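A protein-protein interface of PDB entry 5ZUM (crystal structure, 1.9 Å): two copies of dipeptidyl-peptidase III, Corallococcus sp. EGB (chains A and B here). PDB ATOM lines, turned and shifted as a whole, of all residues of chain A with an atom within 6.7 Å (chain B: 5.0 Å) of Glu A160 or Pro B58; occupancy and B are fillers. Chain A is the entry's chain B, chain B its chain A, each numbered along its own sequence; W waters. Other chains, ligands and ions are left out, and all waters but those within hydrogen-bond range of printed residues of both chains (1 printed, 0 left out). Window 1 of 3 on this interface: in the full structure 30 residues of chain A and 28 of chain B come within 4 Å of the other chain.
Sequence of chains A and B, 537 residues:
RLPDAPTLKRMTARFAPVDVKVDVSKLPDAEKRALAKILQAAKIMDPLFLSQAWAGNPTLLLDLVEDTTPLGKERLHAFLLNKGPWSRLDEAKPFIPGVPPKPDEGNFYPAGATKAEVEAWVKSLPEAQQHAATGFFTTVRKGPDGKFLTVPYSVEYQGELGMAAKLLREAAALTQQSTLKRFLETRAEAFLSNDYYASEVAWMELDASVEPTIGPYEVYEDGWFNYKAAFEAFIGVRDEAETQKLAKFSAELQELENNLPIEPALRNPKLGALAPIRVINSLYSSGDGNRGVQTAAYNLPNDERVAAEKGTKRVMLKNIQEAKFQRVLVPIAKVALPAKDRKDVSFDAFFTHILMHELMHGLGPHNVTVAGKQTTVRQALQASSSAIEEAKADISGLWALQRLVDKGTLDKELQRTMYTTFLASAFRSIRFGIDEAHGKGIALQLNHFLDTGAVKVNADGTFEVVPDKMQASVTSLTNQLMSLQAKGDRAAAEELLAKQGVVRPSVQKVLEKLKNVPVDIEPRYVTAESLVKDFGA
Printed residues of chain B within 4 Å of Ile A44: Thr B59.
Printed residues of chain B within 4 Å of Pro A47: Pro B58 (3.7 Å), Thr B59 (3.3 Å) and Leu B62 (3.6 Å).
Of the printed residues of chain B, Glu A160 touches Ala B55 (3.5 Å) and Pro B58 (3.9 Å).
Ala A165 touches none of the printed residues of chain B.
Asn B57 touches none of the printed residues of chain A.
Among the printed residues, pairs that only touch across the chains: Ile A44 with Thr B59, Pro A47 with Pro B58, Pro A47 with Thr B59, Pro A47 with Leu B62, Leu A61 with Leu B62, Gly A159 with Ala B55, Glu A160 with Ala B55, Glu A160 with Pro B58 and Met A163 with Ala B55.
The backbone NH (N) of Gly B56 sits at hydrogen-bond distance from the side-chain sulfur (SD) of Met A163 (3.4 Å).
Water W1 lies within hydrogen-bond range of the side-chain hydroxyl of Thr B59 (2.6 Å), the backbone carbonyl oxygen of Ala B55 (2.6 Å) and the side-chain carboxylate of Glu A160 (3.0 Å).
Positions printed for both chains: 51, 58 and 61.
Of the 10 pairs that touch across the chains among the printed residues, none has its exchanged pair printed and touching as well.
Printed residues of chain A that touch a printed residue of chain B: Ile A44, Pro A47, Leu A61, Gly A159, Glu A160 and Met A163.
Hydrophobic or aromatic side chains of chain A that line the printed part of chain B: Ile A44, Pro A47, Leu A61 and Met A163.
Along chain A the printed residues that touch a printed residue of chain B span positions 44 to 163.
Hydrophobic or aromatic side chains of chain B within 4 Å of the printed part of chain A: Ala B55, Pro B58 and Leu B62.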
ATOM      1  N   ILE A  44      28.396  -4.565  10.586  1.00  0.00           N
ATOM      2  CA  ILE A  44      27.323  -4.286   9.636  1.00  0.00           C
ATOM      3  C   ILE A  44      27.825  -4.297   8.198  1.00  0.00           C
ATOM      4  O   ILE A  44      27.086  -4.573   7.278  1.00  0.00           O
ATOM      5  CB  ILE A  44      26.629  -2.954   9.978  1.00  0.00           C
ATOM      6  CG1 ILE A  44      25.930  -3.084  11.330  1.00  0.00           C
ATOM      7  CG2 ILE A  44      25.653  -2.579   8.874  1.00  0.00           C
ATOM      8  CD1 ILE A  44      25.442  -1.762  11.886  1.00  0.00           C
ATOM      9  N   MET A  45      29.117  -4.079   7.999  1.00  0.00           N
ATOM     10  CA  MET A  45      29.670  -4.147   6.660  1.00  0.00           C
ATOM     11  C   MET A  45      29.546  -5.545   6.052  1.00  0.00           C
ATOM     12  O   MET A  45      29.515  -5.650   4.834  1.00  0.00           O
ATOM     13  CB  MET A  45      31.095  -3.622   6.548  1.00  0.00           C
ATOM     14  CG  MET A  45      31.320  -2.287   7.267  1.00  0.00           C
ATOM     15  SD  MET A  45      30.306  -0.847   6.391  1.00  0.00           S
ATOM     16  CE  MET A  45      28.881  -0.745   7.734  1.00  0.00           C
ATOM     17  N   PRO A  47      27.019  -8.009   6.237  1.00  0.00           N
ATOM     18  CA  PRO A  47      25.808  -8.265   5.398  1.00  0.00           C
ATOM     19  C   PRO A  47      25.603  -7.275   4.266  1.00  0.00           C
ATOM     20  O   PRO A  47      25.058  -7.633   3.213  1.00  0.00           O
ATOM     21  CB  PRO A  47      24.636  -8.156   6.391  1.00  0.00           C
ATOM     22  CG  PRO A  47      25.176  -7.338   7.525  1.00  0.00           C
ATOM     23  CD  PRO A  47      26.654  -7.759   7.640  1.00  0.00           C
ATOM     24  N   LEU A  48      26.068  -6.043   4.450  1.00  0.00           N
ATOM     25  CA  LEU A  48      26.044  -5.077   3.360  1.00  0.00           C
ATOM     26  C   LEU A  48      26.837  -5.567   2.131  1.00  0.00           C
ATOM     27  O   LEU A  48      26.342  -5.587   0.973  1.00  0.00           O
ATOM     28  CB  LEU A  48      26.559  -3.705   3.815  1.00  0.00           C
ATOM     29  CG  LEU A  48      25.597  -2.690   4.416  1.00  0.00           C
ATOM     30  CD1 LEU A  48      26.367  -1.443   4.858  1.00  0.00           C
ATOM     31  CD2 LEU A  48      24.406  -2.306   3.549  1.00  0.00           C
ATOM     32  N   SER A  51      25.308  -8.646   0.335  1.00  0.00           N
ATOM     33  CA  SER A  51      24.226  -8.351  -0.601  1.00  0.00           C
ATOM     34  C   SER A  51      24.635  -7.494  -1.788  1.00  0.00           C
ATOM     35  O   SER A  51      24.033  -7.575  -2.860  1.00  0.00           O
ATOM     36  CB  SER A  51      23.020  -7.815   0.151  1.00  0.00           C
ATOM     37  OG  SER A  51      22.221  -8.926   0.561  1.00  0.00           O
ATOM     38  N   PRO A  58      21.570 -13.634   0.754  1.00  0.00           N
ATOM     39  CA  PRO A  58      20.785 -13.850   1.973  1.00  0.00           C
ATOM     40  C   PRO A  58      19.877 -15.086   1.893  1.00  0.00           C
ATOM     41  O   PRO A  58      19.815 -15.866   2.774  1.00  0.00           O
ATOM     42  CB  PRO A  58      20.008 -12.552   2.127  1.00  0.00           C
ATOM     43  CG  PRO A  58      20.766 -11.546   1.356  1.00  0.00           C
ATOM     44  CD  PRO A  58      21.382 -12.296   0.215  1.00  0.00           C
ATOM     45  N   LEU A  61      21.992 -18.256   2.277  1.00  0.00           N
ATOM     46  CA  LEU A  61      22.518 -18.448   3.622  1.00  0.00           C
ATOM     47  C   LEU A  61      21.486 -19.215   4.471  1.00  0.00           C
ATOM     48  O   LEU A  61      21.811 -20.203   5.145  1.00  0.00           O
ATOM     49  CB  LEU A  61      22.843 -17.099   4.241  1.00  0.00           C
ATOM     50  CG  LEU A  61      23.191 -17.133   5.740  1.00  0.00           C
ATOM     51  CD1 LEU A  61      24.351 -18.082   6.029  1.00  0.00           C
ATOM     52  CD2 LEU A  61      23.493 -15.735   6.201  1.00  0.00           C
ATOM     53  N   TYR A 157      21.011   1.764   1.052  1.00  0.00           N
ATOM     54  CA  TYR A 157      21.349   1.005   2.244  1.00  0.00           C
ATOM     55  C   TYR A 157      21.009   1.733   3.562  1.00  0.00           C
ATOM     56  O   TYR A 157      21.605   1.512   4.566  1.00  0.00           O
ATOM     57  CB  TYR A 157      22.832   0.653   2.231  1.00  0.00           C
ATOM     58  CG  TYR A 157      23.357   0.133   0.916  1.00  0.00           C
ATOM     59  CD1 TYR A 157      23.094  -1.163   0.499  1.00  0.00           C
ATOM     60  CD2 TYR A 157      24.122   0.918   0.105  1.00  0.00           C
ATOM     61  CE1 TYR A 157      23.567  -1.624  -0.705  1.00  0.00           C
ATOM     62  CE2 TYR A 157      24.579   0.479  -1.100  1.00  0.00           C
ATOM     63  CZ  TYR A 157      24.315  -0.795  -1.517  1.00  0.00           C
ATOM     64  OH  TYR A 157      24.810  -1.222  -2.705  1.00  0.00           O
ATOM     65  N   GLN A 158      19.996   2.555   3.524  1.00  0.00           N
ATOM     66  CA  GLN A 158      19.651   3.379   4.666  1.00  0.00           C
ATOM     67  C   GLN A 158      19.468   2.747   6.037  1.00  0.00           C
ATOM     68  O   GLN A 158      19.955   3.267   6.981  1.00  0.00           O
ATOM     69  CB  GLN A 158      18.490   4.306   4.361  1.00  0.00           C
ATOM     70  CG  GLN A 158      18.258   5.339   5.425  1.00  0.00           C
ATOM     71  CD  GLN A 158      17.649   6.637   4.944  1.00  0.00           C
ATOM     72  OE1 GLN A 158      16.693   7.099   5.507  1.00  0.00           O
ATOM     73  NE2 GLN A 158      18.219   7.218   3.938  1.00  0.00           N
ATOM     74  N   GLY A 159      18.729   1.659   6.120  1.00  0.00           N
ATOM     75  CA  GLY A 159      18.478   1.015   7.377  1.00  0.00           C
ATOM     76  C   GLY A 159      19.763   0.607   8.057  1.00  0.00           C
ATOM     77  O   GLY A 159      20.064   1.014   9.138  1.00  0.00           O
ATOM     78  N   GLU A 160      20.538  -0.180   7.348  1.00  0.00           N
ATOM     79  CA  GLU A 160      21.791  -0.635   7.847  1.00  0.00           C
ATOM     80  C   GLU A 160      22.760   0.513   8.180  1.00  0.00           C
ATOM     81  O   GLU A 160      23.325   0.546   9.213  1.00  0.00           O
ATOM     82  CB  GLU A 160      22.377  -1.705   6.912  1.00  0.00           C
ATOM     83  CG  GLU A 160      21.587  -3.006   6.990  1.00  0.00           C
ATOM     84  CD  GLU A 160      22.060  -4.094   6.043  1.00  0.00           C
ATOM     85  OE1 GLU A 160      22.225  -3.804   4.871  1.00  0.00           O
ATOM     86  OE2 GLU A 160      22.240  -5.218   6.458  1.00  0.00           O
ATOM     87  N   LEU A 161      22.878   1.457   7.280  1.00  0.00           N
ATOM     88  CA  LEU A 161      23.798   2.579   7.454  1.00  0.00           C
ATOM     89  C   LEU A 161      23.371   3.496   8.579  1.00  0.00           C
ATOM     90  O   LEU A 161      24.205   4.009   9.324  1.00  0.00           O
ATOM     91  CB  LEU A 161      23.943   3.369   6.181  1.00  0.00           C
ATOM     92  CG  LEU A 161      24.755   2.699   5.066  1.00  0.00           C
ATOM     93  CD1 LEU A 161      24.725   3.596   3.862  1.00  0.00           C
ATOM     94  CD2 LEU A 161      26.211   2.422   5.484  1.00  0.00           C
ATOM     95  N   GLY A 162      22.065   3.647   8.776  1.00  0.00           N
ATOM     96  CA  GLY A 162      21.580   4.381   9.946  1.00  0.00           C
ATOM     97  C   GLY A 162      22.019   3.750  11.250  1.00  0.00           C
ATOM     98  O   GLY A 162      22.309   4.447  12.229  1.00  0.00           O
ATOM     99  N   MET A 163      22.002   2.428  11.289  1.00  0.00           N
ATOM    100  CA  MET A 163      22.368   1.732  12.525  1.00  0.00           C
ATOM    101  C   MET A 163      23.843   1.823  12.744  1.00  0.00           C
ATOM    102  O   MET A 163      24.302   1.989  13.881  1.00  0.00           O
ATOM    103  CB  MET A 163      22.023   0.273  12.460  1.00  0.00           C
ATOM    104  CG  MET A 163      20.548   0.084  12.701  1.00  0.00           C
ATOM    105  SD  MET A 163      20.417  -1.877  12.777  1.00  0.00           S
ATOM    106  CE  MET A 163      21.684  -2.309  14.221  1.00  0.00           C
ATOM    107  N   ALA A 164      24.598   1.821  11.641  1.00  0.00           N
ATOM    108  CA  ALA A 164      26.048   1.955  11.744  1.00  0.00           C
ATOM    109  C   ALA A 164      26.393   3.367  12.235  1.00  0.00           C
ATOM    110  O   ALA A 164      27.254   3.543  13.099  1.00  0.00           O
ATOM    111  CB  ALA A 164      26.688   1.682  10.390  1.00  0.00           C
ATOM    112  N   ALA A 165      25.743   4.356  11.634  1.00  0.00           N
ATOM    113  CA  ALA A 165      25.905   5.749  12.028  1.00  0.00           C
ATOM    114  C   ALA A 165      25.627   5.975  13.502  1.00  0.00           C
ATOM    115  O   ALA A 165      26.379   6.683  14.174  1.00  0.00           O
ATOM    116  CB  ALA A 165      25.017   6.641  11.193  1.00  0.00           C
ATOM    117  N   PHE A 191      27.481   8.671   5.927  1.00  0.00           N
ATOM    118  CA  PHE A 191      26.664   7.512   5.607  1.00  0.00           C
ATOM    119  C   PHE A 191      25.286   7.959   5.148  1.00  0.00           C
ATOM    120  O   PHE A 191      24.703   7.325   4.244  1.00  0.00           O
ATOM    121  CB  PHE A 191      26.519   6.568   6.792  1.00  0.00           C
ATOM    122  CG  PHE A 191      27.755   5.774   7.132  1.00  0.00           C
ATOM    123  CD1 PHE A 191      28.703   5.465   6.173  1.00  0.00           C
ATOM    124  CD2 PHE A 191      27.812   5.128   8.342  1.00  0.00           C
ATOM    125  CE1 PHE A 191      29.779   4.652   6.488  1.00  0.00           C
ATOM    126  CE2 PHE A 191      28.858   4.284   8.656  1.00  0.00           C
ATOM    127  CZ  PHE A 191      29.871   4.090   7.746  1.00  0.00           C
ATOM    128  N   SER B  51      14.447  -8.340   6.601  1.00  0.00           N
ATOM    129  CA  SER B  51      15.019  -7.015   6.455  1.00  0.00           C
ATOM    130  C   SER B  51      13.994  -5.926   6.666  1.00  0.00           C
ATOM    131  O   SER B  51      14.309  -4.867   7.172  1.00  0.00           O
ATOM    132  CB  SER B  51      15.682  -6.847   5.084  1.00  0.00           C
ATOM    133  OG  SER B  51      16.982  -7.419   5.165  1.00  0.00           O
ATOM    134  N   TRP B  54      13.453  -5.510  10.685  1.00  0.00           N
ATOM    135  CA  TRP B  54      14.496  -4.782  11.424  1.00  0.00           C
ATOM    136  C   TRP B  54      15.747  -4.714  10.562  1.00  0.00           C
ATOM    137  O   TRP B  54      16.235  -5.743  10.133  1.00  0.00           O
ATOM    138  CB  TRP B  54      14.820  -5.501  12.730  1.00  0.00           C
ATOM    139  CG  TRP B  54      15.787  -4.777  13.643  1.00  0.00           C
ATOM    140  CD1 TRP B  54      15.802  -3.451  13.936  1.00  0.00           C
ATOM    141  CD2 TRP B  54      16.842  -5.374  14.408  1.00  0.00           C
ATOM    142  NE1 TRP B  54      16.831  -3.175  14.810  1.00  0.00           N
ATOM    143  CE2 TRP B  54      17.407  -4.355  15.201  1.00  0.00           C
ATOM    144  CE3 TRP B  54      17.257  -6.691  14.610  1.00  0.00           C
ATOM    145  CZ2 TRP B  54      18.503  -4.586  16.041  1.00  0.00           C
ATOM    146  CZ3 TRP B  54      18.301  -6.928  15.476  1.00  0.00           C
ATOM    147  CH2 TRP B  54      18.920  -5.874  16.172  1.00  0.00           C
ATOM    148  N   ALA B  55      16.298  -3.520  10.383  1.00  0.00           N
ATOM    149  CA  ALA B  55      17.570  -3.349   9.653  1.00  0.00           C
ATOM    150  C   ALA B  55      18.732  -4.169  10.255  1.00  0.00           C
ATOM    151  O   ALA B  55      19.657  -4.540   9.522  1.00  0.00           O
ATOM    152  CB  ALA B  55      17.953  -1.886   9.655  1.00  0.00           C
ATOM    153  N   GLY B  56      18.645  -4.449  11.563  1.00  0.00           N
ATOM    154  CA  GLY B  56      19.652  -5.220  12.317  1.00  0.00           C
ATOM    155  C   GLY B  56      19.564  -6.736  12.129  1.00  0.00           C
ATOM    156  O   GLY B  56      20.473  -7.473  12.530  1.00  0.00           O
ATOM    157  N   ASN B  57      18.517  -7.218  11.478  1.00  0.00           N
ATOM    158  CA  ASN B  57      18.377  -8.639  11.307  1.00  0.00           C
ATOM    159  C   ASN B  57      19.479  -9.347  10.529  1.00  0.00           C
ATOM    160  O   ASN B  57      19.917 -10.339  10.957  1.00  0.00           O
ATOM    161  CB  ASN B  57      16.973  -9.051  10.836  1.00  0.00           C
ATOM    162  CG  ASN B  57      15.969  -9.204  12.003  1.00  0.00           C
ATOM    163  OD1 ASN B  57      16.336  -9.424  13.114  1.00  0.00           O
ATOM    164  ND2 ASN B  57      14.717  -9.063  11.707  1.00  0.00           N
ATOM    165  N   PRO B  58      19.919  -8.809   9.384  1.00  0.00           N
ATOM    166  CA  PRO B  58      20.942  -9.589   8.677  1.00  0.00           C
ATOM    167  C   PRO B  58      22.263  -9.674   9.476  1.00  0.00           C
ATOM    168  O   PRO B  58      22.876 -10.732   9.548  1.00  0.00           O
ATOM    169  CB  PRO B  58      21.116  -8.838   7.361  1.00  0.00           C
ATOM    170  CG  PRO B  58      19.804  -8.165   7.137  1.00  0.00           C
ATOM    171  CD  PRO B  58      19.294  -7.806   8.514  1.00  0.00           C
ATOM    172  N   THR B  59      22.677  -8.588  10.109  1.00  0.00           N
ATOM    173  CA  THR B  59      23.885  -8.578  10.953  1.00  0.00           C
ATOM    174  C   THR B  59      23.730  -9.551  12.107  1.00  0.00           C
ATOM    175  O   THR B  59      24.650 -10.325  12.407  1.00  0.00           O
ATOM    176  CB  THR B  59      24.158  -7.160  11.543  1.00  0.00           C
ATOM    177  OG1 THR B  59      24.260  -6.205  10.490  1.00  0.00           O
ATOM    178  CG2 THR B  59      25.433  -7.130  12.370  1.00  0.00           C
ATOM    179  N   LEU B  60      22.603  -9.495  12.816  1.00  0.00           N
ATOM    180  CA  LEU B  60      22.379 -10.470  13.901  1.00  0.00           C
ATOM    181  C   LEU B  60      22.445 -11.934  13.415  1.00  0.00           C
ATOM    182  O   LEU B  60      23.027 -12.799  14.103  1.00  0.00           O
ATOM    183  CB  LEU B  60      21.073 -10.161  14.663  1.00  0.00           C
ATOM    184  CG  LEU B  60      20.652 -11.061  15.820  1.00  0.00           C
ATOM    185  CD1 LEU B  60      21.782 -11.161  16.826  1.00  0.00           C
ATOM    186  CD2 LEU B  60      19.421 -10.530  16.515  1.00  0.00           C
ATOM    187  N   LEU B  61      21.868 -12.221  12.247  1.00  0.00           N
ATOM    188  CA  LEU B  61      21.788 -13.584  11.744  1.00  0.00           C
ATOM    189  C   LEU B  61      23.199 -14.171  11.548  1.00  0.00           C
ATOM    190  O   LEU B  61      23.456 -15.307  11.929  1.00  0.00           O
ATOM    191  CB  LEU B  61      21.015 -13.655  10.433  1.00  0.00           C
ATOM    192  CG  LEU B  61      21.036 -14.997   9.693  1.00  0.00           C
ATOM    193  CD1 LEU B  61      20.553 -16.115  10.601  1.00  0.00           C
ATOM    194  CD2 LEU B  61      20.231 -14.915   8.409  1.00  0.00           C
ATOM    195  N   LEU B  62      24.125 -13.359  11.038  1.00  0.00           N
ATOM    196  CA  LEU B  62      25.507 -13.785  10.898  1.00  0.00           C
ATOM    197  C   LEU B  62      26.184 -14.076  12.252  1.00  0.00           C
ATOM    198  O   LEU B  62      26.934 -15.036  12.328  1.00  0.00           O
ATOM    199  CB  LEU B  62      26.328 -12.766  10.073  1.00  0.00           C
ATOM    200  CG  LEU B  62      25.968 -12.620   8.594  1.00  0.00           C
ATOM    201  CD1 LEU B  62      26.507 -11.339   7.973  1.00  0.00           C
ATOM    202  CD2 LEU B  62      26.411 -13.827   7.790  1.00  0.00           C
HETATM  203  O   HOH W   1      21.950  -5.792   9.419  1.00  0.00           O
